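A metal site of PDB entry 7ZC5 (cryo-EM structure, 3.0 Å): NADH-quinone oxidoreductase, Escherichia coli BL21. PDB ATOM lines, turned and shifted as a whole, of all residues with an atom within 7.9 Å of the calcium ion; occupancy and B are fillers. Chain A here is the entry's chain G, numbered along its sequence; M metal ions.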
ATOM      1  N   GLU A 615      16.750  -7.127  21.238  1.00  0.00           N
ATOM      2  CA  GLU A 615      18.003  -6.381  21.205  1.00  0.00           C
ATOM      3  C   GLU A 615      17.808  -4.880  21.358  1.00  0.00           C
ATOM      4  O   GLU A 615      18.724  -4.123  21.042  1.00  0.00           O
ATOM      5  CB  GLU A 615      18.750  -6.687  19.909  1.00  0.00           C
ATOM      6  CG  GLU A 615      19.012  -8.142  19.645  1.00  0.00           C
ATOM      7  CD  GLU A 615      18.313  -8.647  18.417  1.00  0.00           C
ATOM      8  OE1 GLU A 615      17.671  -7.844  17.713  1.00  0.00           O
ATOM      9  OE2 GLU A 615      18.409  -9.861  18.131  1.00  0.00           O
ATOM     10  N   SER A 616      16.654  -4.438  21.835  1.00  0.00           N
ATOM     11  CA  SER A 616      16.368  -3.010  21.864  1.00  0.00           C
ATOM     12  C   SER A 616      15.467  -2.672  23.047  1.00  0.00           C
ATOM     13  O   SER A 616      14.828  -3.548  23.642  1.00  0.00           O
ATOM     14  CB  SER A 616      15.697  -2.544  20.577  1.00  0.00           C
ATOM     15  OG  SER A 616      14.478  -3.214  20.367  1.00  0.00           O
ATOM     16  N   ASP A 617      15.438  -1.391  23.378  1.00  0.00           N
ATOM     17  CA  ASP A 617      14.487  -0.817  24.325  1.00  0.00           C
ATOM     18  C   ASP A 617      13.472   0.029  23.580  1.00  0.00           C
ATOM     19  O   ASP A 617      13.692   0.425  22.434  1.00  0.00           O
ATOM     20  CB  ASP A 617      15.207   0.041  25.369  1.00  0.00           C
ATOM     21  CG  ASP A 617      16.515  -0.557  25.811  1.00  0.00           C
ATOM     22  OD1 ASP A 617      16.491  -1.480  26.639  1.00  0.00           O
ATOM     23  OD2 ASP A 617      17.571  -0.109  25.318  1.00  0.00           O
ATOM     24  N   GLY A 618      12.353   0.306  24.234  1.00  0.00           N
ATOM     25  CA  GLY A 618      11.385   1.176  23.620  1.00  0.00           C
ATOM     26  C   GLY A 618      10.079   1.160  24.389  1.00  0.00           C
ATOM     27  O   GLY A 618       9.974   0.580  25.463  1.00  0.00           O
ATOM     28  N   PHE A 631      12.466  -3.555  27.623  1.00  0.00           N
ATOM     29  CA  PHE A 631      13.890  -3.362  27.828  1.00  0.00           C
ATOM     30  C   PHE A 631      14.665  -4.382  27.016  1.00  0.00           C
ATOM     31  O   PHE A 631      14.148  -5.432  26.631  1.00  0.00           O
ATOM     32  CB  PHE A 631      14.252  -3.463  29.305  1.00  0.00           C
ATOM     33  CG  PHE A 631      13.451  -2.573  30.196  1.00  0.00           C
ATOM     34  CD1 PHE A 631      12.244  -2.996  30.728  1.00  0.00           C
ATOM     35  CD2 PHE A 631      13.883  -1.308  30.507  1.00  0.00           C
ATOM     36  CE1 PHE A 631      11.513  -2.178  31.536  1.00  0.00           C
ATOM     37  CE2 PHE A 631      13.147  -0.485  31.321  1.00  0.00           C
ATOM     38  CZ  PHE A 631      11.969  -0.930  31.835  1.00  0.00           C
ATOM     39  N   GLN A 632      15.912  -4.040  26.731  1.00  0.00           N
ATOM     40  CA  GLN A 632      16.769  -4.902  25.944  1.00  0.00           C
ATOM     41  C   GLN A 632      17.110  -6.159  26.731  1.00  0.00           C
ATOM     42  O   GLN A 632      17.372  -6.105  27.937  1.00  0.00           O
ATOM     43  CB  GLN A 632      18.043  -4.153  25.561  1.00  0.00           C
ATOM     44  CG  GLN A 632      18.964  -4.888  24.651  1.00  0.00           C
ATOM     45  CD  GLN A 632      20.118  -4.026  24.224  1.00  0.00           C
ATOM     46  OE1 GLN A 632      20.205  -2.866  24.603  1.00  0.00           O
ATOM     47  NE2 GLN A 632      21.010  -4.571  23.423  1.00  0.00           N
ATOM     48  N   VAL A 633      17.112  -7.299  26.045  1.00  0.00           N
ATOM     49  CA  VAL A 633      17.410  -8.552  26.712  1.00  0.00           C
ATOM     50  C   VAL A 633      18.907  -8.787  26.756  1.00  0.00           C
ATOM     51  O   VAL A 633      19.468  -9.138  27.800  1.00  0.00           O
ATOM     52  CB  VAL A 633      16.679  -9.716  26.024  1.00  0.00           C
ATOM     53  CG1 VAL A 633      16.855 -10.982  26.820  1.00  0.00           C
ATOM     54  CG2 VAL A 633      15.216  -9.385  25.891  1.00  0.00           C
ATOM     55  N   TYR A 634      19.591  -8.564  25.636  1.00  0.00           N
ATOM     56  CA  TYR A 634      20.999  -8.887  25.555  1.00  0.00           C
ATOM     57  C   TYR A 634      21.682  -7.936  24.583  1.00  0.00           C
ATOM     58  O   TYR A 634      21.039  -7.264  23.788  1.00  0.00           O
ATOM     59  CB  TYR A 634      21.233 -10.324  25.093  1.00  0.00           C
ATOM     60  CG  TYR A 634      20.674 -10.646  23.728  1.00  0.00           C
ATOM     61  CD1 TYR A 634      19.340 -10.972  23.574  1.00  0.00           C
ATOM     62  CD2 TYR A 634      21.487 -10.645  22.614  1.00  0.00           C
ATOM     63  CE1 TYR A 634      18.819 -11.258  22.336  1.00  0.00           C
ATOM     64  CE2 TYR A 634      20.983 -10.928  21.371  1.00  0.00           C
ATOM     65  CZ  TYR A 634      19.640 -11.237  21.242  1.00  0.00           C
ATOM     66  OH  TYR A 634      19.128 -11.536  20.008  1.00  0.00           O
ATOM     67  N   ASP A 635      23.006  -7.891  24.675  1.00  0.00           N
ATOM     68  CA  ASP A 635      23.817  -7.164  23.725  1.00  0.00           C
ATOM     69  C   ASP A 635      24.114  -8.055  22.533  1.00  0.00           C
ATOM     70  O   ASP A 635      24.721  -9.117  22.708  1.00  0.00           O
ATOM     71  CB  ASP A 635      25.110  -6.704  24.360  1.00  0.00           C
ATOM     72  CG  ASP A 635      25.696  -5.485  23.686  1.00  0.00           C
ATOM     73  OD1 ASP A 635      26.094  -5.593  22.504  1.00  0.00           O
ATOM     74  OD2 ASP A 635      25.753  -4.426  24.335  1.00  0.00           O
ATOM     75  N   PRO A 636      23.711  -7.680  21.317  1.00  0.00           N
ATOM     76  CA  PRO A 636      24.028  -8.507  20.147  1.00  0.00           C
ATOM     77  C   PRO A 636      25.512  -8.584  19.834  1.00  0.00           C
ATOM     78  O   PRO A 636      25.946  -9.553  19.208  1.00  0.00           O
ATOM     79  CB  PRO A 636      23.265  -7.838  19.014  1.00  0.00           C
ATOM     80  CG  PRO A 636      22.429  -6.783  19.634  1.00  0.00           C
ATOM     81  CD  PRO A 636      23.019  -6.442  20.945  1.00  0.00           C
ATOM     82  N   LEU A 646      21.901  -1.784  16.119  1.00  0.00           N
ATOM     83  CA  LEU A 646      21.489  -0.773  17.075  1.00  0.00           C
ATOM     84  C   LEU A 646      19.978  -0.624  17.063  1.00  0.00           C
ATOM     85  O   LEU A 646      19.281  -1.115  16.189  1.00  0.00           O
ATOM     86  CB  LEU A 646      22.167   0.565  16.755  1.00  0.00           C
ATOM     87  CG  LEU A 646      23.679   0.488  16.673  1.00  0.00           C
ATOM     88  CD1 LEU A 646      24.244   1.769  16.147  1.00  0.00           C
ATOM     89  CD2 LEU A 646      24.230   0.195  18.053  1.00  0.00           C
ATOM     90  N   GLU A 647      19.488   0.079  18.084  1.00  0.00           N
ATOM     91  CA  GLU A 647      18.082   0.443  18.131  1.00  0.00           C
ATOM     92  C   GLU A 647      17.728   1.331  16.946  1.00  0.00           C
ATOM     93  O   GLU A 647      18.558   2.081  16.452  1.00  0.00           O
ATOM     94  CB  GLU A 647      17.770   1.157  19.436  1.00  0.00           C
ATOM     95  CG  GLU A 647      17.868   0.299  20.676  1.00  0.00           C
ATOM     96  CD  GLU A 647      19.255   0.217  21.251  1.00  0.00           C
ATOM     97  OE1 GLU A 647      20.215   0.669  20.593  1.00  0.00           O
ATOM     98  OE2 GLU A 647      19.399  -0.281  22.386  1.00  0.00           O
ATOM     99  N   TRP A 649      15.625   3.869  16.818  1.00  0.00           N
ATOM    100  CA  TRP A 649      15.664   5.275  17.191  1.00  0.00           C
ATOM    101  C   TRP A 649      17.089   5.779  17.344  1.00  0.00           C
ATOM    102  O   TRP A 649      17.349   6.948  17.071  1.00  0.00           O
ATOM    103  CB  TRP A 649      14.882   5.514  18.468  1.00  0.00           C
ATOM    104  CG  TRP A 649      15.198   4.569  19.559  1.00  0.00           C
ATOM    105  CD1 TRP A 649      14.581   3.391  19.821  1.00  0.00           C
ATOM    106  CD2 TRP A 649      16.208   4.715  20.563  1.00  0.00           C
ATOM    107  NE1 TRP A 649      15.142   2.788  20.914  1.00  0.00           N
ATOM    108  CE2 TRP A 649      16.145   3.593  21.392  1.00  0.00           C
ATOM    109  CE3 TRP A 649      17.160   5.701  20.836  1.00  0.00           C
ATOM    110  CZ2 TRP A 649      16.987   3.417  22.473  1.00  0.00           C
ATOM    111  CZ3 TRP A 649      18.000   5.520  21.904  1.00  0.00           C
ATOM    112  CH2 TRP A 649      17.916   4.384  22.712  1.00  0.00           C
ATOM    113  N   ARG A 650      18.010   4.919  17.751  1.00  0.00           N
ATOM    114  CA  ARG A 650      19.418   5.308  17.833  1.00  0.00           C
ATOM    115  C   ARG A 650      19.986   5.576  16.447  1.00  0.00           C
ATOM    116  O   ARG A 650      20.653   6.602  16.236  1.00  0.00           O
ATOM    117  CB  ARG A 650      20.202   4.206  18.543  1.00  0.00           C
ATOM    118  CG  ARG A 650      21.691   4.460  18.639  1.00  0.00           C
ATOM    119  CD  ARG A 650      22.282   3.713  19.806  1.00  0.00           C
ATOM    120  NE  ARG A 650      22.068   4.402  21.074  1.00  0.00           N
ATOM    121  CZ  ARG A 650      21.509   3.857  22.141  1.00  0.00           C
ATOM    122  NH1 ARG A 650      21.075   2.614  22.126  1.00  0.00           N
ATOM    123  NH2 ARG A 650      21.401   4.576  23.252  1.00  0.00           N
ATOM    124  N   LEU A 669      18.107   6.601  25.636  1.00  0.00           N
ATOM    125  CA  LEU A 669      16.675   6.372  25.472  1.00  0.00           C
ATOM    126  C   LEU A 669      15.841   7.449  26.137  1.00  0.00           C
ATOM    127  O   LEU A 669      14.822   7.892  25.588  1.00  0.00           O
ATOM    128  CB  LEU A 669      16.301   4.997  26.022  1.00  0.00           C
ATOM    129  CG  LEU A 669      14.815   4.664  26.078  1.00  0.00           C
ATOM    130  CD1 LEU A 669      14.280   4.450  24.685  1.00  0.00           C
ATOM    131  CD2 LEU A 669      14.562   3.456  26.932  1.00  0.00           C
ATOM    132  N   ARG A 704      19.641  -8.374  35.326  1.00  0.00           N
ATOM    133  CA  ARG A 704      19.007  -9.067  34.209  1.00  0.00           C
ATOM    134  C   ARG A 704      19.135 -10.575  34.290  1.00  0.00           C
ATOM    135  O   ARG A 704      18.297 -11.282  33.740  1.00  0.00           O
ATOM    136  CB  ARG A 704      19.591  -8.596  32.880  1.00  0.00           C
ATOM    137  CG  ARG A 704      18.881  -7.426  32.267  1.00  0.00           C
ATOM    138  CD  ARG A 704      19.248  -7.290  30.811  1.00  0.00           C
ATOM    139  NE  ARG A 704      18.669  -6.098  30.212  1.00  0.00           N
ATOM    140  CZ  ARG A 704      19.315  -4.941  30.072  1.00  0.00           C
ATOM    141  NH1 ARG A 704      20.562  -4.796  30.502  1.00  0.00           N
ATOM    142  NH2 ARG A 704      18.710  -3.921  29.492  1.00  0.00           N
ATOM    143  N   GLN A 728      27.669  -2.409  28.721  1.00  0.00           N
ATOM    144  CA  GLN A 728      27.178  -1.245  29.443  1.00  0.00           C
ATOM    145  C   GLN A 728      25.809  -0.867  28.921  1.00  0.00           C
ATOM    146  O   GLN A 728      25.606  -0.747  27.705  1.00  0.00           O
ATOM    147  CB  GLN A 728      28.144  -0.077  29.312  1.00  0.00           C
ATOM    148  CG  GLN A 728      29.435  -0.251  30.094  1.00  0.00           C
ATOM    149  CD  GLN A 728      29.190  -0.828  31.474  1.00  0.00           C
ATOM    150  OE1 GLN A 728      29.584  -1.957  31.763  1.00  0.00           O
ATOM    151  NE2 GLN A 728      28.557  -0.049  32.337  1.00  0.00           N
ATOM    152  N   ASP A 729      24.862  -0.684  29.837  1.00  0.00           N
ATOM    153  CA  ASP A 729      23.502  -0.296  29.504  1.00  0.00           C
ATOM    154  C   ASP A 729      23.294   1.130  30.014  1.00  0.00           C
ATOM    155  O   ASP A 729      22.939   1.341  31.173  1.00  0.00           O
ATOM    156  CB  ASP A 729      22.490  -1.253  30.122  1.00  0.00           C
ATOM    157  CG  ASP A 729      21.099  -1.072  29.550  1.00  0.00           C
ATOM    158  OD1 ASP A 729      20.971  -0.918  28.321  1.00  0.00           O
ATOM    159  OD2 ASP A 729      20.137  -1.110  30.331  1.00  0.00           O
ATOM    160  N   ILE A 730      23.532   2.103  29.134  1.00  0.00           N
ATOM    161  CA  ILE A 730      23.254   3.486  29.479  1.00  0.00           C
ATOM    162  C   ILE A 730      21.785   3.840  29.338  1.00  0.00           C
ATOM    163  O   ILE A 730      21.355   4.869  29.850  1.00  0.00           O
ATOM    164  CB  ILE A 730      24.072   4.469  28.610  1.00  0.00           C
ATOM    165  CG1 ILE A 730      23.767   4.232  27.132  1.00  0.00           C
ATOM    166  CG2 ILE A 730      25.547   4.313  28.882  1.00  0.00           C
ATOM    167  CD1 ILE A 730      24.311   5.291  26.231  1.00  0.00           C
ATOM    168  N   ASP A 731      21.011   2.992  28.666  1.00  0.00           N
ATOM    169  CA  ASP A 731      19.633   3.356  28.340  1.00  0.00           C
ATOM    170  C   ASP A 731      18.685   3.108  29.494  1.00  0.00           C
ATOM    171  O   ASP A 731      17.779   3.912  29.736  1.00  0.00           O
ATOM    172  CB  ASP A 731      19.177   2.588  27.108  1.00  0.00           C
ATOM    173  CG  ASP A 731      20.017   2.888  25.895  1.00  0.00           C
ATOM    174  OD1 ASP A 731      20.513   4.020  25.792  1.00  0.00           O
ATOM    175  OD2 ASP A 731      20.193   1.994  25.062  1.00  0.00           O
ATOM    176  N   THR A 732      18.837   2.001  30.208  1.00  0.00           N
ATOM    177  CA  THR A 732      17.857   1.599  31.200  1.00  0.00           C
ATOM    178  C   THR A 732      18.505   1.429  32.572  1.00  0.00           C
ATOM    179  O   THR A 732      19.716   1.499  32.735  1.00  0.00           O
ATOM    180  CB  THR A 732      17.151   0.286  30.825  1.00  0.00           C
ATOM    181  OG1 THR A 732      17.992  -0.819  31.159  1.00  0.00           O
ATOM    182  CG2 THR A 732      16.848   0.237  29.341  1.00  0.00           C
ATOM    183  N   PHE A 736      23.504  -5.517  32.482  1.00  0.00           N
ATOM    184  CA  PHE A 736      23.745  -6.746  31.730  1.00  0.00           C
ATOM    185  C   PHE A 736      24.586  -7.731  32.527  1.00  0.00           C
ATOM    186  O   PHE A 736      25.576  -8.254  32.013  1.00  0.00           O
ATOM    187  CB  PHE A 736      24.460  -6.455  30.418  1.00  0.00           C
ATOM    188  CG  PHE A 736      23.597  -5.875  29.357  1.00  0.00           C
ATOM    189  CD1 PHE A 736      22.628  -6.639  28.730  1.00  0.00           C
ATOM    190  CD2 PHE A 736      23.768  -4.560  28.941  1.00  0.00           C
ATOM    191  CE1 PHE A 736      21.838  -6.102  27.739  1.00  0.00           C
ATOM    192  CE2 PHE A 736      22.985  -4.023  27.956  1.00  0.00           C
ATOM    193  CZ  PHE A 736      22.022  -4.790  27.352  1.00  0.00           C
HETATM  194 CA    CA M   1      19.996  -0.454  24.825  1.00  0.00          CA
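Residues that only touch the calcium ion: Asp 729.
Five residues have an atom within 4 Å of the calcium ion: Asp 617, Gln 632, Glu 647, Asp 729 and Asp 731.
OE1 of Gln 632 is bound to the calcium ion (2.4 Å).
The side-chain carboxylate (OD2) of Asp 731 binds the calcium ion, 2.5 Å away.
OD2 of Asp 617 is bound to the calcium ion, 2.5 Å away.
OE2 of Glu 647 is bound to the calcium ion.
NH1 of Arg 650 is in salt-bridge range of OE1 of Glu 647 (2.6 Å).
The backbone carbonyl oxygen (O) of Asp 617 is in hydrogen-bond range of the indole nitrogen (NE1) of Trp 649, 3.2 Å away.
O of Tyr 634 is in hydrogen-bond range of NE2 of Gln 632 (2.7 Å).
NH2 of Arg 704 lies within salt-bridge range of OD2 of Asp 729.
NE2 of Gln 632 is in hydrogen-bond range of O of Glu 615, 3.3 Å away.
The backbone carbonyl oxygen (O) of Gln 632 lies within hydrogen-bond range of the guanidinium group (NE) of Arg 704.
OD1 of Asp 731 lies within salt-bridge range of NH2 of Arg 650 (2.7 Å).
The backbone NH (N) of Thr 732 lies close to the side-chain carboxylate (OD2) of Asp 729 (3.4 Å).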
